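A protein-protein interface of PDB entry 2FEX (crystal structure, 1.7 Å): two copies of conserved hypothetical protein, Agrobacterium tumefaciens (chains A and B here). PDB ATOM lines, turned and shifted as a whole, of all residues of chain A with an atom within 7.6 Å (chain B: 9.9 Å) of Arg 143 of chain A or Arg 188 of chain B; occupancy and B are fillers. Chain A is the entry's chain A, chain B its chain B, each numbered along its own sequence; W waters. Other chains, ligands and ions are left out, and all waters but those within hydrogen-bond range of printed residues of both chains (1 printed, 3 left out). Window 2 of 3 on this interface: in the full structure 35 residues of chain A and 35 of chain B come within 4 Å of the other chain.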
ATOM      1  N   HIS A 118      -4.982 -17.620  14.262  1.00  0.00           N
ATOM      2  CA  HIS A 118      -5.659 -17.384  12.958  1.00  0.00           C
ATOM      3  C   HIS A 118      -7.168 -17.556  13.137  1.00  0.00           C
ATOM      4  O   HIS A 118      -7.636 -17.956  14.203  1.00  0.00           O
ATOM      5  CB  HIS A 118      -5.174 -18.399  11.931  1.00  0.00           C
ATOM      6  CG  HIS A 118      -5.437 -19.828  12.343  1.00  0.00           C
ATOM      7  ND1 HIS A 118      -4.535 -20.583  13.072  1.00  0.00           N
ATOM      8  CD2 HIS A 118      -6.536 -20.599  12.178  1.00  0.00           C
ATOM      9  CE1 HIS A 118      -5.083 -21.756  13.367  1.00  0.00           C
ATOM     10  NE2 HIS A 118      -6.306 -21.787  12.846  1.00  0.00           N
ATOM     11  N   THR A 119      -7.919 -17.221  12.086  1.00  0.00           N
ATOM     12  CA  THR A 119      -9.337 -17.477  12.076  1.00  0.00           C
ATOM     13  C   THR A 119      -9.704 -17.879  10.628  1.00  0.00           C
ATOM     14  O   THR A 119      -8.818 -18.247   9.818  1.00  0.00           O
ATOM     15  CB  THR A 119     -10.149 -16.264  12.589  1.00  0.00           C
ATOM     16  OG1 THR A 119     -11.532 -16.624  12.809  1.00  0.00           O
ATOM     17  CG2 THR A 119     -10.022 -15.049  11.614  1.00  0.00           C
ATOM     18  N   GLY A 120     -11.004 -17.908  10.362  1.00  0.00           N
ATOM     19  CA  GLY A 120     -11.479 -18.409   9.046  1.00  0.00           C
ATOM     20  C   GLY A 120     -12.983 -18.250   9.033  1.00  0.00           C
ATOM     21  O   GLY A 120     -13.603 -17.590   9.932  1.00  0.00           O
ATOM     22  N   ARG A 139      -9.067 -18.905  16.423  1.00  0.00           N
ATOM     23  CA  ARG A 139      -9.841 -17.885  17.167  1.00  0.00           C
ATOM     24  C   ARG A 139     -11.215 -17.708  16.549  1.00  0.00           C
ATOM     25  O   ARG A 139     -11.352 -17.223  15.421  1.00  0.00           O
ATOM     26  CB  ARG A 139      -9.091 -16.569  17.193  1.00  0.00           C
ATOM     27  CG  ARG A 139      -7.810 -16.724  17.936  1.00  0.00           C
ATOM     28  CD  ARG A 139      -7.189 -15.407  18.305  1.00  0.00           C
ATOM     29  NE  ARG A 139      -5.994 -15.734  19.096  1.00  0.00           N
ATOM     30  CZ  ARG A 139      -4.979 -14.898  19.334  1.00  0.00           C
ATOM     31  NH1 ARG A 139      -4.992 -13.657  18.837  1.00  0.00           N
ATOM     32  NH2 ARG A 139      -3.939 -15.321  20.056  1.00  0.00           N
ATOM     33  N   ASP A 140     -12.244 -18.120  17.290  1.00  0.00           N
ATOM     34  CA  ASP A 140     -13.609 -17.967  16.784  1.00  0.00           C
ATOM     35  C   ASP A 140     -14.093 -16.552  17.177  1.00  0.00           C
ATOM     36  O   ASP A 140     -14.654 -16.345  18.261  1.00  0.00           O
ATOM     37  CB  ASP A 140     -14.517 -19.066  17.367  1.00  0.00           C
ATOM     38  CG  ASP A 140     -15.931 -19.010  16.814  1.00  0.00           C
ATOM     39  OD1 ASP A 140     -16.139 -18.519  15.676  1.00  0.00           O
ATOM     40  OD2 ASP A 140     -16.858 -19.477  17.544  1.00  0.00           O
ATOM     41  N   GLN A 141     -13.825 -15.584  16.311  1.00  0.00           N
ATOM     42  CA  GLN A 141     -14.156 -14.162  16.559  1.00  0.00           C
ATOM     43  C   GLN A 141     -14.491 -13.537  15.206  1.00  0.00           C
ATOM     44  O   GLN A 141     -14.072 -14.104  14.177  1.00  0.00           O
ATOM     45  CB  GLN A 141     -12.937 -13.434  17.140  1.00  0.00           C
ATOM     46  CG  GLN A 141     -11.662 -13.422  16.174  1.00  0.00           C
ATOM     47  CD  GLN A 141     -10.494 -12.666  16.752  1.00  0.00           C
ATOM     48  OE1 GLN A 141     -10.066 -12.936  17.904  1.00  0.00           O
ATOM     49  NE2 GLN A 141      -9.980 -11.679  15.992  1.00  0.00           N
ATOM     50  N   PRO A 142     -15.246 -12.412  15.182  1.00  0.00           N
ATOM     51  CA  PRO A 142     -15.636 -11.858  13.875  1.00  0.00           C
ATOM     52  C   PRO A 142     -14.538 -11.131  13.108  1.00  0.00           C
ATOM     53  O   PRO A 142     -14.645 -11.018  11.884  1.00  0.00           O
ATOM     54  CB  PRO A 142     -16.784 -10.873  14.200  1.00  0.00           C
ATOM     55  CG  PRO A 142     -16.555 -10.523  15.676  1.00  0.00           C
ATOM     56  CD  PRO A 142     -15.890 -11.701  16.311  1.00  0.00           C
ATOM     57  N   ARG A 143     -13.535 -10.609  13.803  1.00  0.00           N
ATOM     58  CA  ARG A 143     -12.531  -9.754  13.097  1.00  0.00           C
ATOM     59  C   ARG A 143     -11.323 -10.576  12.659  1.00  0.00           C
ATOM     60  O   ARG A 143     -11.000 -11.616  13.253  1.00  0.00           O
ATOM     61  CB  ARG A 143     -12.074  -8.580  13.964  1.00  0.00           C
ATOM     62  CG  ARG A 143     -13.244  -7.580  14.259  1.00  0.00           C
ATOM     63  CD  ARG A 143     -12.728  -6.518  15.175  1.00  0.00           C
ATOM     64  NE  ARG A 143     -13.830  -5.668  15.593  1.00  0.00           N
ATOM     65  CZ  ARG A 143     -13.702  -4.376  15.852  1.00  0.00           C
ATOM     66  NH1 ARG A 143     -12.504  -3.796  15.744  1.00  0.00           N
ATOM     67  NH2 ARG A 143     -14.775  -3.668  16.204  1.00  0.00           N
ATOM     68  N   ALA A 144     -10.622 -10.071  11.631  1.00  0.00           N
ATOM     69  CA  ALA A 144      -9.375 -10.690  11.151  1.00  0.00           C
ATOM     70  C   ALA A 144      -8.362 -10.890  12.268  1.00  0.00           C
ATOM     71  O   ALA A 144      -8.320 -10.101  13.271  1.00  0.00           O
ATOM     72  CB  ALA A 144      -8.727  -9.801  10.089  1.00  0.00           C
ATOM     73  N   VAL A 145      -7.521 -11.892  12.088  1.00  0.00           N
ATOM     74  CA  VAL A 145      -6.432 -12.173  13.014  1.00  0.00           C
ATOM     75  C   VAL A 145      -5.086 -12.007  12.294  1.00  0.00           C
ATOM     76  O   VAL A 145      -4.940 -12.344  11.091  1.00  0.00           O
ATOM     77  CB  VAL A 145      -6.578 -13.580  13.541  1.00  0.00           C
ATOM     78  CG1 VAL A 145      -5.310 -14.047  14.370  1.00  0.00           C
ATOM     79  CG2 VAL A 145      -7.821 -13.712  14.391  1.00  0.00           C
ATOM     80  N   SER A 146      -4.135 -11.425  13.018  1.00  0.00           N
ATOM     81  CA  SER A 146      -2.759 -11.305  12.518  1.00  0.00           C
ATOM     82  C   SER A 146      -1.778 -11.874  13.539  1.00  0.00           C
ATOM     83  O   SER A 146      -1.729 -11.400  14.710  1.00  0.00           O
ATOM     84  CB  SER A 146      -2.427  -9.841  12.265  1.00  0.00           C
ATOM     85  OG  SER A 146      -1.119  -9.747  11.727  1.00  0.00           O
ATOM     86  N   THR A 152      -5.426 -13.725   8.607  1.00  0.00           N
ATOM     87  CA  THR A 152      -6.559 -14.508   8.162  1.00  0.00           C
ATOM     88  C   THR A 152      -7.875 -13.812   8.569  1.00  0.00           C
ATOM     89  O   THR A 152      -7.906 -13.019   9.494  1.00  0.00           O
ATOM     90  CB  THR A 152      -6.514 -15.964   8.731  1.00  0.00           C
ATOM     91  OG1 THR A 152      -6.318 -15.889  10.155  1.00  0.00           O
ATOM     92  CG2 THR A 152      -5.372 -16.778   8.020  1.00  0.00           C
ATOM     93  N   ALA A 153      -8.944 -14.129   7.830  1.00  0.00           N
ATOM     94  CA  ALA A 153     -10.279 -13.585   8.094  1.00  0.00           C
ATOM     95  C   ALA A 153     -11.328 -14.426   7.432  1.00  0.00           C
ATOM     96  O   ALA A 153     -11.059 -15.162   6.471  1.00  0.00           O
ATOM     97  CB  ALA A 153     -10.358 -12.176   7.519  1.00  0.00           C
ATOM     98  N   ALA A 154     -12.546 -14.284   7.972  1.00  0.00           N
ATOM     99  CA  ALA A 154     -13.726 -14.876   7.344  1.00  0.00           C
ATOM    100  C   ALA A 154     -14.082 -13.915   6.174  1.00  0.00           C
ATOM    101  O   ALA A 154     -13.714 -12.705   6.206  1.00  0.00           O
ATOM    102  CB  ALA A 154     -14.827 -14.890   8.359  1.00  0.00           C
ATOM    103  N   SER A 156     -16.800 -12.589   5.798  1.00  0.00           N
ATOM    104  CA  SER A 156     -17.614 -11.503   6.379  1.00  0.00           C
ATOM    105  C   SER A 156     -16.786 -10.327   6.950  1.00  0.00           C
ATOM    106  O   SER A 156     -17.377  -9.351   7.474  1.00  0.00           O
ATOM    107  CB  SER A 156     -18.460 -12.095   7.529  1.00  0.00           C
ATOM    108  OG  SER A 156     -17.595 -12.816   8.425  1.00  0.00           O
ATOM    109  N   ALA A 157     -15.447 -10.434   6.916  1.00  0.00           N
ATOM    110  CA  ALA A 157     -14.603  -9.423   7.599  1.00  0.00           C
ATOM    111  C   ALA A 157     -13.622  -8.734   6.618  1.00  0.00           C
ATOM    112  O   ALA A 157     -12.418  -8.675   6.916  1.00  0.00           O
ATOM    113  CB  ALA A 157     -13.811 -10.078   8.754  1.00  0.00           C
ATOM    114  N   SER A 160     -11.573  -5.521   8.451  1.00  0.00           N
ATOM    115  CA  SER A 160     -10.485  -5.817   9.366  1.00  0.00           C
ATOM    116  C   SER A 160      -9.360  -6.611   8.651  1.00  0.00           C
ATOM    117  O   SER A 160      -8.205  -6.491   9.032  1.00  0.00           O
ATOM    118  CB  SER A 160     -10.961  -6.532  10.623  1.00  0.00           C
ATOM    119  OG  SER A 160     -11.667  -7.724  10.298  1.00  0.00           O
ATOM    120  N   PHE A 161      -9.739  -7.350   7.614  1.00  0.00           N
ATOM    121  CA  PHE A 161      -8.712  -8.030   6.779  1.00  0.00           C
ATOM    122  C   PHE A 161      -7.778  -6.944   6.196  1.00  0.00           C
ATOM    123  O   PHE A 161      -6.526  -7.031   6.324  1.00  0.00           O
ATOM    124  CB  PHE A 161      -9.404  -8.795   5.658  1.00  0.00           C
ATOM    125  CG  PHE A 161      -8.467  -9.673   4.832  1.00  0.00           C
ATOM    126  CD1 PHE A 161      -7.695 -10.665   5.428  1.00  0.00           C
ATOM    127  CD2 PHE A 161      -8.423  -9.494   3.436  1.00  0.00           C
ATOM    128  CE1 PHE A 161      -6.899 -11.545   4.611  1.00  0.00           C
ATOM    129  CE2 PHE A 161      -7.623 -10.370   2.607  1.00  0.00           C
ATOM    130  CZ  PHE A 161      -6.829 -11.352   3.223  1.00  0.00           C
ATOM    131  N   GLU A 164      -5.625  -5.221   8.962  1.00  0.00           N
ATOM    132  CA  GLU A 164      -4.519  -6.037   9.523  1.00  0.00           C
ATOM    133  C   GLU A 164      -3.362  -6.181   8.509  1.00  0.00           C
ATOM    134  O   GLU A 164      -2.193  -6.234   8.908  1.00  0.00           O
ATOM    135  CB  GLU A 164      -4.997  -7.416   9.980  1.00  0.00           C
ATOM    136  CG  GLU A 164      -5.935  -7.369  11.190  1.00  0.00           C
ATOM    137  CD  GLU A 164      -5.247  -6.854  12.483  1.00  0.00           C
ATOM    138  OE1 GLU A 164      -3.978  -6.724  12.567  1.00  0.00           O
ATOM    139  OE2 GLU A 164      -6.001  -6.549  13.438  1.00  0.00           O
ATOM    140  N   ALA A 184     -18.080   1.187   9.599  1.00  0.00           N
ATOM    141  CA  ALA A 184     -18.848   0.670  10.730  1.00  0.00           C
ATOM    142  C   ALA A 184     -20.196   1.336  10.841  1.00  0.00           C
ATOM    143  O   ALA A 184     -21.165   0.735  11.378  1.00  0.00           O
ATOM    144  CB  ALA A 184     -18.072   0.899  12.096  1.00  0.00           C
ATOM    145  N   GLU A 186     -22.676   2.223   9.045  1.00  0.00           N
ATOM    146  CA  GLU A 186     -23.916   1.690   8.419  1.00  0.00           C
ATOM    147  C   GLU A 186     -24.438   0.443   9.164  1.00  0.00           C
ATOM    148  O   GLU A 186     -25.509  -0.058   8.799  1.00  0.00           O
ATOM    149  CB  GLU A 186     -23.779   1.369   6.917  1.00  0.00           C
ATOM    150  CG  GLU A 186     -22.822   0.233   6.589  1.00  0.00           C
ATOM    151  CD  GLU A 186     -23.042  -0.284   5.160  1.00  0.00           C
ATOM    152  OE1 GLU A 186     -24.155  -0.173   4.666  1.00  0.00           O
ATOM    153  OE2 GLU A 186     -22.106  -0.803   4.561  1.00  0.00           O
ATOM    154  N   HIS A 187     -23.657  -0.065  10.139  1.00  0.00           N
ATOM    155  CA  HIS A 187     -24.056  -1.261  10.903  1.00  0.00           C
ATOM    156  C   HIS A 187     -24.501  -0.913  12.337  1.00  0.00           C
ATOM    157  O   HIS A 187     -24.912  -1.790  13.105  1.00  0.00           O
ATOM    158  CB  HIS A 187     -22.942  -2.293  10.879  1.00  0.00           C
ATOM    159  CG  HIS A 187     -22.548  -2.714   9.498  1.00  0.00           C
ATOM    160  ND1 HIS A 187     -23.345  -3.523   8.701  1.00  0.00           N
ATOM    161  CD2 HIS A 187     -21.454  -2.433   8.770  1.00  0.00           C
ATOM    162  CE1 HIS A 187     -22.748  -3.709   7.542  1.00  0.00           C
ATOM    163  NE2 HIS A 187     -21.581  -3.080   7.566  1.00  0.00           N
ATOM    164  N   ARG A 188     -24.388   0.378  12.631  1.00  0.00           N
ATOM    165  CA  ARG A 188     -24.955   1.134  13.761  1.00  0.00           C
ATOM    166  C   ARG A 188     -23.879   1.597  14.713  1.00  0.00           C
ATOM    167  O   ARG A 188     -23.342   2.696  14.515  1.00  0.00           O
ATOM    168  CB  ARG A 188     -26.203   0.539  14.408  1.00  0.00           C
ATOM    169  CG  ARG A 188     -27.376   0.630  13.508  1.00  0.00           C
ATOM    170  CD  ARG A 188     -28.647   1.028  14.315  1.00  0.00           C
ATOM    171  N   ARG B 143     -26.913   4.888   6.520  1.00  0.00           N
ATOM    172  CA  ARG B 143     -27.327   3.832   5.580  1.00  0.00           C
ATOM    173  C   ARG B 143     -27.922   4.346   4.267  1.00  0.00           C
ATOM    174  O   ARG B 143     -28.428   5.477   4.180  1.00  0.00           O
ATOM    175  CB  ARG B 143     -28.320   2.839   6.204  1.00  0.00           C
ATOM    176  CG  ARG B 143     -27.759   2.108   7.485  1.00  0.00           C
ATOM    177  CD  ARG B 143     -28.869   1.353   8.162  1.00  0.00           C
ATOM    178  NE  ARG B 143     -28.399   0.858   9.456  1.00  0.00           N
ATOM    179  CZ  ARG B 143     -28.640  -0.381   9.896  1.00  0.00           C
ATOM    180  NH1 ARG B 143     -29.348  -1.223   9.148  1.00  0.00           N
ATOM    181  NH2 ARG B 143     -28.158  -0.800  11.072  1.00  0.00           N
ATOM    182  N   LEU B 180     -26.134 -11.363   2.943  1.00  0.00           N
ATOM    183  CA  LEU B 180     -25.777  -9.942   3.138  1.00  0.00           C
ATOM    184  C   LEU B 180     -25.759  -9.485   4.610  1.00  0.00           C
ATOM    185  O   LEU B 180     -25.232  -8.414   4.898  1.00  0.00           O
ATOM    186  CB  LEU B 180     -26.708  -8.993   2.322  1.00  0.00           C
ATOM    187  CG  LEU B 180     -26.600  -9.229   0.810  1.00  0.00           C
ATOM    188  CD1 LEU B 180     -27.578  -8.355   0.108  1.00  0.00           C
ATOM    189  CD2 LEU B 180     -25.195  -8.964   0.329  1.00  0.00           C
ATOM    190  N   GLN B 181     -26.344 -10.262   5.532  1.00  0.00           N
ATOM    191  CA  GLN B 181     -26.425  -9.835   6.964  1.00  0.00           C
ATOM    192  C   GLN B 181     -25.128 -10.062   7.775  1.00  0.00           C
ATOM    193  O   GLN B 181     -25.029  -9.644   8.934  1.00  0.00           O
ATOM    194  CB  GLN B 181     -27.607 -10.522   7.699  1.00  0.00           C
ATOM    195  CG  GLN B 181     -27.386 -12.047   7.858  1.00  0.00           C
ATOM    196  CD  GLN B 181     -28.602 -12.807   8.423  1.00  0.00           C
ATOM    197  OE1 GLN B 181     -29.684 -12.237   8.603  1.00  0.00           O
ATOM    198  NE2 GLN B 181     -28.410 -14.102   8.714  1.00  0.00           N
ATOM    199  N   ILE B 182     -24.117 -10.636   7.121  1.00  0.00           N
ATOM    200  CA  ILE B 182     -22.947 -11.192   7.848  1.00  0.00           C
ATOM    201  C   ILE B 182     -21.894 -10.110   8.138  1.00  0.00           C
ATOM    202  O   ILE B 182     -20.962 -10.341   8.902  1.00  0.00           O
ATOM    203  CB  ILE B 182     -22.315 -12.348   7.051  1.00  0.00           C
ATOM    204  CG1 ILE B 182     -21.750 -11.894   5.681  1.00  0.00           C
ATOM    205  CG2 ILE B 182     -23.335 -13.478   6.852  1.00  0.00           C
ATOM    206  CD1 ILE B 182     -20.963 -13.023   4.883  1.00  0.00           C
ATOM    207  N   PHE B 183     -22.037  -8.972   7.465  1.00  0.00           N
ATOM    208  CA  PHE B 183     -20.998  -7.894   7.454  1.00  0.00           C
ATOM    209  C   PHE B 183     -20.952  -6.969   8.649  1.00  0.00           C
ATOM    210  O   PHE B 183     -19.987  -6.219   8.846  1.00  0.00           O
ATOM    211  CB  PHE B 183     -21.082  -7.128   6.128  1.00  0.00           C
ATOM    212  CG  PHE B 183     -20.751  -8.003   4.971  1.00  0.00           C
ATOM    213  CD1 PHE B 183     -19.384  -8.316   4.708  1.00  0.00           C
ATOM    214  CD2 PHE B 183     -21.749  -8.610   4.212  1.00  0.00           C
ATOM    215  CE1 PHE B 183     -19.037  -9.164   3.629  1.00  0.00           C
ATOM    216  CE2 PHE B 183     -21.421  -9.493   3.175  1.00  0.00           C
ATOM    217  CZ  PHE B 183     -20.031  -9.758   2.879  1.00  0.00           C
ATOM    218  N   ALA B 184     -21.982  -7.037   9.504  1.00  0.00           N
ATOM    219  CA  ALA B 184     -22.045  -6.153  10.654  1.00  0.00           C
ATOM    220  C   ALA B 184     -21.128  -6.628  11.792  1.00  0.00           C
ATOM    221  O   ALA B 184     -20.637  -5.811  12.577  1.00  0.00           O
ATOM    222  CB  ALA B 184     -23.493  -6.109  11.177  1.00  0.00           C
ATOM    223  N   ALA B 185     -20.942  -7.948  11.889  1.00  0.00           N
ATOM    224  CA  ALA B 185     -20.307  -8.550  13.074  1.00  0.00           C
ATOM    225  C   ALA B 185     -18.903  -7.987  13.327  1.00  0.00           C
ATOM    226  O   ALA B 185     -18.516  -7.786  14.488  1.00  0.00           O
ATOM    227  CB  ALA B 185     -20.292 -10.090  12.945  1.00  0.00           C
ATOM    228  N   GLU B 186     -18.147  -7.679  12.257  1.00  0.00           N
ATOM    229  CA  GLU B 186     -16.761  -7.230  12.464  1.00  0.00           C
ATOM    230  C   GLU B 186     -16.706  -5.758  12.941  1.00  0.00           C
ATOM    231  O   GLU B 186     -15.616  -5.260  13.261  1.00  0.00           O
ATOM    232  CB  GLU B 186     -15.873  -7.404  11.216  1.00  0.00           C
ATOM    233  CG  GLU B 186     -16.291  -6.493  10.050  1.00  0.00           C
ATOM    234  CD  GLU B 186     -15.188  -6.385   8.983  1.00  0.00           C
ATOM    235  OE1 GLU B 186     -14.023  -6.514   9.358  1.00  0.00           O
ATOM    236  OE2 GLU B 186     -15.486  -6.183   7.800  1.00  0.00           O
ATOM    237  N   HIS B 187     -17.879  -5.127  13.010  1.00  0.00           N
ATOM    238  CA  HIS B 187     -17.972  -3.723  13.463  1.00  0.00           C
ATOM    239  C   HIS B 187     -18.506  -3.565  14.881  1.00  0.00           C
ATOM    240  O   HIS B 187     -18.586  -2.446  15.397  1.00  0.00           O
ATOM    241  CB  HIS B 187     -18.707  -2.845  12.439  1.00  0.00           C
ATOM    242  CG  HIS B 187     -18.062  -2.857  11.089  1.00  0.00           C
ATOM    243  ND1 HIS B 187     -16.868  -2.213  10.832  1.00  0.00           N
ATOM    244  CD2 HIS B 187     -18.428  -3.460   9.937  1.00  0.00           C
ATOM    245  CE1 HIS B 187     -16.531  -2.421   9.567  1.00  0.00           C
ATOM    246  NE2 HIS B 187     -17.460  -3.183   9.004  1.00  0.00           N
ATOM    247  N   ARG B 188     -18.891  -4.673  15.492  1.00  0.00           N
ATOM    248  CA  ARG B 188     -19.395  -4.648  16.895  1.00  0.00           C
ATOM    249  C   ARG B 188     -18.301  -4.427  17.935  1.00  0.00           C
ATOM    250  O   ARG B 188     -17.138  -4.793  17.730  1.00  0.00           O
ATOM    251  CB  ARG B 188     -20.126  -5.952  17.230  1.00  0.00           C
ATOM    252  CG  ARG B 188     -21.371  -6.150  16.387  1.00  0.00           C
ATOM    253  CD  ARG B 188     -21.811  -4.842  15.764  1.00  0.00           C
ATOM    254  NE  ARG B 188     -22.862  -5.007  14.774  1.00  0.00           N
ATOM    255  CZ  ARG B 188     -24.071  -4.464  14.876  1.00  0.00           C
ATOM    256  NH1 ARG B 188     -24.384  -3.706  15.925  1.00  0.00           N
ATOM    257  NH2 ARG B 188     -24.967  -4.675  13.923  1.00  0.00           N
HETATM  258  O   HOH W   1     -26.693   2.362  11.000  1.00  0.00           O
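NE of Arg 143 of chain A sits at hydrogen-bond distance from O of Glu 186 of chain B, at 3.0 Å.
The backbone carbonyl oxygen (O) of Arg 188 of chain B is in hydrogen-bond range of the guanidinium group (NH2) of Arg 143 of chain A (3.0 Å).
The side-chain carboxylate (OE1) of Glu 186 of chain B lies within hydrogen-bond range of the backbone NH (N) of Ser 160 of chain A (2.8 Å).
The backbone carbonyl oxygen (O) of Glu 186 of chain A lies within hydrogen-bond range of the guanidinium group (NE) of Arg 143 of chain B (3.1 Å).
The backbone carbonyl oxygen (O) of His 187 of chain A lies within hydrogen-bond range of the guanidinium group (NH2) of Arg 188 of chain B (3.0 Å).
The side-chain amide nitrogen of Gln 141 of chain A is in hydrogen-bond range of the backbone carbonyl oxygen of Arg 143 of chain A, at 2.9 Å.
The backbone NH of Ala 144 of chain A is in hydrogen-bond range of the side-chain hydroxyl of Ser 160 of chain A, at 2.9 Å.
The guanidinium group of Arg 188 of chain B lies within hydrogen-bond range of the backbone carbonyl oxygen of Ala 184 of chain B (3.2 Å).
O of Ala 185 of chain B touches CB of Pro 142 of chain A, 3.6 Å away.
Arg 143 of chain A touches His 187 of chain B (NH2 to C, 3.96 Å).
Ser 156 of chain A touches Ile 182 of chain B (CB to O, 3.3 Å).
Ser 156 of chain A touches Phe 183 of chain B (O to CD1, 3.6 Å).
Glu 186 of chain B touches Ser 156 of chain A.
Ala 157 of chain A touches Glu 186 of chain B.
His 187 of chain B touches Ala 184 of chain A (ND1 to CA, 3.5 Å).
His 187 of chain A touches Arg 143 of chain B (C to NH2, 3.9 Å).
Phe 183 of chain B touches His 187 of chain A.
Arg 188 of chain A touches Arg 143 of chain B.
Arg 143 of chain A touches just these residues of chain B: Glu 186, His 187 and Arg 188.
Arg 188 of chain B touches two residues of chain A.
Printed residues of chain B within 4 Å of Pro 142 of chain A: Ala 185 and Glu 186.
No residue of chain B comes within 4 Å of Ala 144 of chain A.
Of the printed residues of chain A, Ala 184 of chain B touches His 187.
Of the printed residues of chain B, Glu 186 of chain A touches Arg 143.
Of the printed residues of chain A, Ile 182 of chain B touches Ser 156 (3.3 Å).
Printed residues of chain B within 4 Å of Arg 188 of chain A: Arg 143 (2.9 Å).
Of the 10 printed residues of chain B, 8 touch a printed residue of chain A.
Hydrophobic or aromatic side chains of chain B that line the printed part of chain A: Ile 182, Phe 183, Ala 184, Ala 185 and His 187.
Printed residues of chain A that touch a printed residue of chain B: Pro 142, Arg 143, Ser 156, Ala 157, Ser 160, Ala 184, Glu 186, His 187 and Arg 188.
Hydrophobic or aromatic side chains of chain A within 4 Å of the printed part of chain B: Pro 142, Ala 157, Ala 184 and His 187.
Among the printed residues, no Asp or Glu carboxylate lies within 4 Å of a Lys or Arg side-chain nitrogen of the other chain.
Arg 143 of chain A touches Glu 186 of chain B, and with the chains exchanged Glu 186 of chain A touches Arg 143 of chain B.
Arg 143 of chain A touches His 187 of chain B, and with the chains exchanged His 187 of chain A touches Arg 143 of chain B.
His 187 of chain A touches its own counterpart, His 187 of chain B.
His 187 of chain A touches Arg 188 of chain B, but with the chains exchanged Arg 188 of chain A does not touch His 187 of chain B (6.5 Å).
Water W1 lies within hydrogen-bond range of NE of Arg 143 of chain B (2.7 Å), N of Arg 188 of chain A (3.5 Å) and O of Glu 186 of chain A (3.5 Å).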
